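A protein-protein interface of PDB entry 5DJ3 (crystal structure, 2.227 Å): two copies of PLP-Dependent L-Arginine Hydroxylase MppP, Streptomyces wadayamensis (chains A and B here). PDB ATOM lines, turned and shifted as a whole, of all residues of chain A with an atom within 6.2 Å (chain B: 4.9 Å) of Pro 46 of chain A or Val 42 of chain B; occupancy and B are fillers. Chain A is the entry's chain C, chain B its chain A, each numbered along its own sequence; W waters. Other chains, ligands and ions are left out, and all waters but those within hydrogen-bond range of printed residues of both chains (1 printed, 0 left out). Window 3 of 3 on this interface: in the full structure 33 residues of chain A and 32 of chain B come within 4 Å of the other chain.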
ATOM      1  N   VAL A  42      25.385 -29.461 -21.151  1.00  0.00           N
ATOM      2  CA  VAL A  42      25.027 -28.371 -22.049  1.00  0.00           C
ATOM      3  C   VAL A  42      23.953 -28.838 -23.020  1.00  0.00           C
ATOM      4  O   VAL A  42      23.020 -28.094 -23.328  1.00  0.00           O
ATOM      5  CB  VAL A  42      26.291 -27.852 -22.769  1.00  0.00           C
ATOM      6  CG1 VAL A  42      25.943 -26.997 -23.972  1.00  0.00           C
ATOM      7  CG2 VAL A  42      27.184 -27.054 -21.764  1.00  0.00           C
ATOM      8  N   ASN A  43      24.065 -30.088 -23.499  1.00  0.00           N
ATOM      9  CA  ASN A  43      23.039 -30.688 -24.344  1.00  0.00           C
ATOM     10  C   ASN A  43      21.671 -30.710 -23.685  1.00  0.00           C
ATOM     11  O   ASN A  43      20.670 -30.730 -24.396  1.00  0.00           O
ATOM     12  CB  ASN A  43      23.430 -32.119 -24.735  1.00  0.00           C
ATOM     13  CG  ASN A  43      24.582 -32.149 -25.734  1.00  0.00           C
ATOM     14  OD1 ASN A  43      24.930 -31.118 -26.295  1.00  0.00           O
ATOM     15  ND2 ASN A  43      25.184 -33.310 -25.937  1.00  0.00           N
ATOM     16  N   GLU A  44      21.593 -30.680 -22.353  1.00  0.00           N
ATOM     17  CA  GLU A  44      20.316 -30.727 -21.655  1.00  0.00           C
ATOM     18  C   GLU A  44      19.918 -29.376 -21.074  1.00  0.00           C
ATOM     19  O   GLU A  44      19.094 -29.308 -20.155  1.00  0.00           O
ATOM     20  CB  GLU A  44      20.379 -31.807 -20.578  1.00  0.00           C
ATOM     21  CG  GLU A  44      20.427 -33.197 -21.207  1.00  0.00           C
ATOM     22  CD  GLU A  44      20.687 -34.288 -20.203  1.00  0.00           C
ATOM     23  OE1 GLU A  44      20.463 -34.043 -18.999  1.00  0.00           O
ATOM     24  OE2 GLU A  44      21.129 -35.379 -20.624  1.00  0.00           O
ATOM     25  N   LEU A  45      20.475 -28.296 -21.626  1.00  0.00           N
ATOM     26  CA  LEU A  45      20.057 -26.959 -21.231  1.00  0.00           C
ATOM     27  C   LEU A  45      18.567 -26.743 -21.372  1.00  0.00           C
ATOM     28  O   LEU A  45      18.007 -26.025 -20.531  1.00  0.00           O
ATOM     29  CB  LEU A  45      20.812 -25.899 -22.043  1.00  0.00           C
ATOM     30  CG  LEU A  45      22.125 -25.449 -21.422  1.00  0.00           C
ATOM     31  CD1 LEU A  45      22.987 -24.727 -22.444  1.00  0.00           C
ATOM     32  CD2 LEU A  45      21.845 -24.564 -20.215  1.00  0.00           C
ATOM     33  N   PRO A  46      17.874 -27.276 -22.389  1.00  0.00           N
ATOM     34  CA  PRO A  46      16.402 -27.111 -22.422  1.00  0.00           C
ATOM     35  C   PRO A  46      15.713 -27.760 -21.245  1.00  0.00           C
ATOM     36  O   PRO A  46      14.681 -27.251 -20.798  1.00  0.00           O
ATOM     37  CB  PRO A  46      15.992 -27.771 -23.747  1.00  0.00           C
ATOM     38  CG  PRO A  46      17.283 -27.816 -24.569  1.00  0.00           C
ATOM     39  CD  PRO A  46      18.402 -27.902 -23.620  1.00  0.00           C
ATOM     40  N   VAL A  47      16.238 -28.892 -20.752  1.00  0.00           N
ATOM     41  CA  VAL A  47      15.678 -29.537 -19.566  1.00  0.00           C
ATOM     42  C   VAL A  47      15.906 -28.670 -18.334  1.00  0.00           C
ATOM     43  O   VAL A  47      14.983 -28.450 -17.538  1.00  0.00           O
ATOM     44  CB  VAL A  47      16.269 -30.943 -19.378  1.00  0.00           C
ATOM     45  CG1 VAL A  47      15.607 -31.614 -18.200  1.00  0.00           C
ATOM     46  CG2 VAL A  47      16.089 -31.781 -20.638  1.00  0.00           C
ATOM     47  N   LEU A  48      17.135 -28.158 -18.158  1.00  0.00           N
ATOM     48  CA  LEU A  48      17.375 -27.239 -17.055  1.00  0.00           C
ATOM     49  C   LEU A  48      16.477 -26.024 -17.162  1.00  0.00           C
ATOM     50  O   LEU A  48      16.045 -25.479 -16.138  1.00  0.00           O
ATOM     51  CB  LEU A  48      18.850 -26.789 -17.009  1.00  0.00           C
ATOM     52  CG  LEU A  48      19.904 -27.884 -16.725  1.00  0.00           C
ATOM     53  CD1 LEU A  48      21.265 -27.219 -16.469  1.00  0.00           C
ATOM     54  CD2 LEU A  48      19.560 -28.834 -15.552  1.00  0.00           C
ATOM     55  N   TRP A  49      16.179 -25.584 -18.384  1.00  0.00           N
ATOM     56  CA  TRP A  49      15.287 -24.442 -18.539  1.00  0.00           C
ATOM     57  C   TRP A  49      13.906 -24.791 -18.029  1.00  0.00           C
ATOM     58  O   TRP A  49      13.318 -24.039 -17.251  1.00  0.00           O
ATOM     59  CB  TRP A  49      15.248 -23.995 -19.996  1.00  0.00           C
ATOM     60  CG  TRP A  49      14.522 -22.703 -20.235  1.00  0.00           C
ATOM     61  CD1 TRP A  49      13.181 -22.492 -20.148  1.00  0.00           C
ATOM     62  CD2 TRP A  49      15.096 -21.456 -20.648  1.00  0.00           C
ATOM     63  NE1 TRP A  49      12.884 -21.193 -20.447  1.00  0.00           N
ATOM     64  CE2 TRP A  49      14.042 -20.528 -20.751  1.00  0.00           C
ATOM     65  CE3 TRP A  49      16.400 -21.028 -20.914  1.00  0.00           C
ATOM     66  CZ2 TRP A  49      14.245 -19.193 -21.130  1.00  0.00           C
ATOM     67  CZ3 TRP A  49      16.610 -19.699 -21.271  1.00  0.00           C
ATOM     68  CH2 TRP A  49      15.531 -18.792 -21.376  1.00  0.00           C
ATOM     69  N   ALA A  50      13.404 -25.973 -18.413  1.00  0.00           N
ATOM     70  CA  ALA A  50      12.111 -26.459 -17.928  1.00  0.00           C
ATOM     71  C   ALA A  50      12.081 -26.500 -16.406  1.00  0.00           C
ATOM     72  O   ALA A  50      11.115 -26.052 -15.778  1.00  0.00           O
ATOM     73  CB  ALA A  50      11.818 -27.854 -18.515  1.00  0.00           C
ATOM     74  N   GLU A  51      13.136 -27.044 -15.803  1.00  0.00           N
ATOM     75  CA  GLU A  51      13.219 -27.122 -14.354  1.00  0.00           C
ATOM     76  C   GLU A  51      13.177 -25.731 -13.724  1.00  0.00           C
ATOM     77  O   GLU A  51      12.475 -25.505 -12.730  1.00  0.00           O
ATOM     78  CB  GLU A  51      14.503 -27.856 -13.948  1.00  0.00           C
ATOM     79  CG  GLU A  51      14.629 -28.008 -12.439  1.00  0.00           C
ATOM     80  CD  GLU A  51      15.920 -28.623 -12.011  1.00  0.00           C
ATOM     81  OE1 GLU A  51      16.680 -29.037 -12.889  1.00  0.00           O
ATOM     82  OE2 GLU A  51      16.167 -28.682 -10.800  1.00  0.00           O
ATOM     83  N   LEU B  34       6.571 -19.486 -22.359  1.00  0.00           N
ATOM     84  CA  LEU B  34       7.208 -19.197 -23.636  1.00  0.00           C
ATOM     85  C   LEU B  34       6.219 -19.357 -24.785  1.00  0.00           C
ATOM     86  O   LEU B  34       5.383 -20.265 -24.788  1.00  0.00           O
ATOM     87  CB  LEU B  34       8.389 -20.147 -23.846  1.00  0.00           C
ATOM     88  CG  LEU B  34       9.565 -19.897 -22.909  1.00  0.00           C
ATOM     89  CD1 LEU B  34      10.575 -21.015 -22.995  1.00  0.00           C
ATOM     90  CD2 LEU B  34      10.219 -18.583 -23.253  1.00  0.00           C
ATOM     91  N   GLN B  38       9.752 -18.755 -29.018  1.00  0.00           N
ATOM     92  CA  GLN B  38      10.746 -18.675 -27.951  1.00  0.00           C
ATOM     93  C   GLN B  38      11.118 -20.059 -27.439  1.00  0.00           C
ATOM     94  O   GLN B  38      12.290 -20.322 -27.134  1.00  0.00           O
ATOM     95  CB  GLN B  38      10.221 -17.799 -26.817  1.00  0.00           C
ATOM     96  CG  GLN B  38      10.089 -16.315 -27.225  1.00  0.00           C
ATOM     97  CD  GLN B  38       9.173 -15.524 -26.310  1.00  0.00           C
ATOM     98  OE1 GLN B  38       8.392 -16.105 -25.524  1.00  0.00           O
ATOM     99  NE2 GLN B  38       9.250 -14.186 -26.405  1.00  0.00           N
ATOM    100  N   GLN B  39      10.141 -20.964 -27.345  1.00  0.00           N
ATOM    101  CA  GLN B  39      10.465 -22.330 -26.961  1.00  0.00           C
ATOM    102  C   GLN B  39      11.481 -22.930 -27.924  1.00  0.00           C
ATOM    103  O   GLN B  39      12.394 -23.658 -27.511  1.00  0.00           O
ATOM    104  CB  GLN B  39       9.199 -23.193 -26.913  1.00  0.00           C
ATOM    105  CG  GLN B  39       9.477 -24.611 -26.444  1.00  0.00           C
ATOM    106  CD  GLN B  39      10.024 -24.631 -25.021  1.00  0.00           C
ATOM    107  OE1 GLN B  39       9.405 -24.098 -24.097  1.00  0.00           O
ATOM    108  NE2 GLN B  39      11.195 -25.224 -24.848  1.00  0.00           N
ATOM    109  N   LYS B  40      11.343 -22.623 -29.214  1.00  0.00           N
ATOM    110  CA  LYS B  40      12.281 -23.123 -30.207  1.00  0.00           C
ATOM    111  C   LYS B  40      13.680 -22.552 -29.991  1.00  0.00           C
ATOM    112  O   LYS B  40      14.666 -23.260 -30.205  1.00  0.00           O
ATOM    113  CB  LYS B  40      11.734 -22.813 -31.609  1.00  0.00           C
ATOM    114  CG  LYS B  40      12.552 -23.332 -32.774  1.00  0.00           C
ATOM    115  CD  LYS B  40      11.891 -22.908 -34.116  1.00  0.00           C
ATOM    116  CE  LYS B  40      12.710 -23.298 -35.369  1.00  0.00           C
ATOM    117  NZ  LYS B  40      13.978 -22.501 -35.538  1.00  0.00           N
ATOM    118  N   ILE B  41      13.796 -21.296 -29.539  1.00  0.00           N
ATOM    119  CA  ILE B  41      15.116 -20.753 -29.222  1.00  0.00           C
ATOM    120  C   ILE B  41      15.713 -21.493 -28.046  1.00  0.00           C
ATOM    121  O   ILE B  41      16.905 -21.806 -28.041  1.00  0.00           O
ATOM    122  CB  ILE B  41      15.054 -19.237 -28.943  1.00  0.00           C
ATOM    123  CG1 ILE B  41      14.661 -18.461 -30.213  1.00  0.00           C
ATOM    124  CG2 ILE B  41      16.431 -18.728 -28.404  1.00  0.00           C
ATOM    125  CD1 ILE B  41      14.235 -17.015 -29.942  1.00  0.00           C
ATOM    126  N   VAL B  42      14.905 -21.774 -27.024  1.00  0.00           N
ATOM    127  CA  VAL B  42      15.397 -22.551 -25.889  1.00  0.00           C
ATOM    128  C   VAL B  42      15.852 -23.927 -26.351  1.00  0.00           C
ATOM    129  O   VAL B  42      16.826 -24.488 -25.825  1.00  0.00           O
ATOM    130  CB  VAL B  42      14.328 -22.658 -24.774  1.00  0.00           C
ATOM    131  CG1 VAL B  42      14.721 -23.722 -23.746  1.00  0.00           C
ATOM    132  CG2 VAL B  42      14.189 -21.362 -24.041  1.00  0.00           C
ATOM    133  N   ASN B  43      15.162 -24.508 -27.328  1.00  0.00           N
ATOM    134  CA  ASN B  43      15.593 -25.836 -27.752  1.00  0.00           C
ATOM    135  C   ASN B  43      16.944 -25.807 -28.437  1.00  0.00           C
ATOM    136  O   ASN B  43      17.589 -26.846 -28.534  1.00  0.00           O
ATOM    137  CB  ASN B  43      14.582 -26.483 -28.685  1.00  0.00           C
ATOM    138  CG  ASN B  43      13.298 -26.846 -27.972  1.00  0.00           C
ATOM    139  OD1 ASN B  43      13.295 -27.076 -26.768  1.00  0.00           O
ATOM    140  ND2 ASN B  43      12.205 -26.898 -28.712  1.00  0.00           N
ATOM    141  N   GLU B  44      17.383 -24.652 -28.912  1.00  0.00           N
ATOM    142  CA  GLU B  44      18.652 -24.540 -29.604  1.00  0.00           C
ATOM    143  C   GLU B  44      19.744 -23.999 -28.697  1.00  0.00           C
ATOM    144  O   GLU B  44      20.816 -23.624 -29.183  1.00  0.00           O
ATOM    145  CB  GLU B  44      18.491 -23.653 -30.850  1.00  0.00           C
ATOM    146  CG  GLU B  44      17.625 -24.267 -31.957  1.00  0.00           C
ATOM    147  CD  GLU B  44      17.427 -23.331 -33.156  1.00  0.00           C
ATOM    148  OE1 GLU B  44      18.254 -22.411 -33.366  1.00  0.00           O
ATOM    149  OE2 GLU B  44      16.430 -23.508 -33.889  1.00  0.00           O
ATOM    150  N   LEU B  45      19.510 -23.956 -27.389  1.00  0.00           N
ATOM    151  CA  LEU B  45      20.554 -23.463 -26.497  1.00  0.00           C
ATOM    152  C   LEU B  45      21.882 -24.183 -26.679  1.00  0.00           C
ATOM    153  O   LEU B  45      22.922 -23.510 -26.651  1.00  0.00           O
ATOM    154  CB  LEU B  45      20.084 -23.560 -25.047  1.00  0.00           C
ATOM    155  CG  LEU B  45      19.408 -22.308 -24.538  1.00  0.00           C
ATOM    156  CD1 LEU B  45      18.876 -22.634 -23.152  1.00  0.00           C
ATOM    157  CD2 LEU B  45      20.365 -21.130 -24.483  1.00  0.00           C
ATOM    158  N   PRO B  46      21.929 -25.493 -26.916  1.00  0.00           N
ATOM    159  CA  PRO B  46      23.227 -26.124 -27.204  1.00  0.00           C
ATOM    160  C   PRO B  46      23.898 -25.622 -28.469  1.00  0.00           C
ATOM    161  O   PRO B  46      25.137 -25.649 -28.532  1.00  0.00           O
ATOM    162  CB  PRO B  46      22.881 -27.620 -27.332  1.00  0.00           C
ATOM    163  CG  PRO B  46      21.541 -27.770 -26.714  1.00  0.00           C
ATOM    164  CD  PRO B  46      20.827 -26.465 -26.895  1.00  0.00           C
HETATM  165  O   HOH W   1      12.577 -26.568 -22.181  1.00  0.00           O
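Among the printed residues, pairs that only touch across the chains: Val 42 of chain A with Pro 46 of chain B (3.7 Å), Asn 43 of chain A with Pro 46 of chain B (3.9 Å), Leu 45 of chain A with Leu 45 of chain B (3.9 Å), Pro 46 of chain A with Val 42 of chain B (3.6 Å), Trp 49 of chain A with Leu 34 of chain B (3.4 Å), Trp 49 of chain A with Val 42 of chain B (3.4 Å) and Trp 49 of chain A with Leu 45 of chain B (3.7 Å).
Of the printed residues of chain A, Val 42 of chain B touches Pro 46 and Trp 49. Printed residues of chain B within 4 Å of Trp 49 of chain A: Leu 34 (3.4 Å), Val 42 (3.4 Å) and Leu 45 (3.7 Å). Of the printed residues of chain B, Val 42 of chain A touches Pro 46. Of the printed residues of chain A, Leu 45 of chain B touches Leu 45 (3.9 Å) and Trp 49 (3.7 Å). Leu 48 of chain A touches none of the printed residues of chain B. The nearest residue of chain B that does not touch Pro 46 of chain A is Asn 43 of chain B (4.1 Å). The nearest residue of chain A that does not touch Val 42 of chain B is Leu 45 of chain A (5.1 Å). The nearest printed residue of chain B that does not touch Val 42 of chain A is Leu 45 of chain B (5.3 Å).
Of the 10 printed residues of chain B, 4 touch a printed residue of chain A. Printed residues of chain B that touch a printed residue of chain A: Leu 34, Val 42, Leu 45 and Pro 46. Hydrophobic or aromatic side chains of chain B that line the printed part of chain A: Leu 34, Val 42, Leu 45 and Pro 46. Among the printed residues, no Asp or Glu carboxylate lies within 4 Å of a Lys or Arg side-chain nitrogen of the other chain.
Val 42 of chain A touches Pro 46 of chain B, and with the chains exchanged Pro 46 of chain A touches Val 42 of chain B. Asn 43 of chain A touches Pro 46 of chain B, but with the chains exchanged Pro 46 of chain A does not touch Asn 43 of chain B (4.1 Å). Leu 45 of chain B touches its own counterpart, Leu 45 of chain A. Positions printed for both chains: 42, 43, 44, 45 and 46.
Water W1 lies within hydrogen-bond range of the backbone carbonyl oxygen (O) of Pro 46 of chain A (2.6 Å) and the side-chain amide nitrogen (NE2) of Gln 39 of chain B (3.3 Å).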
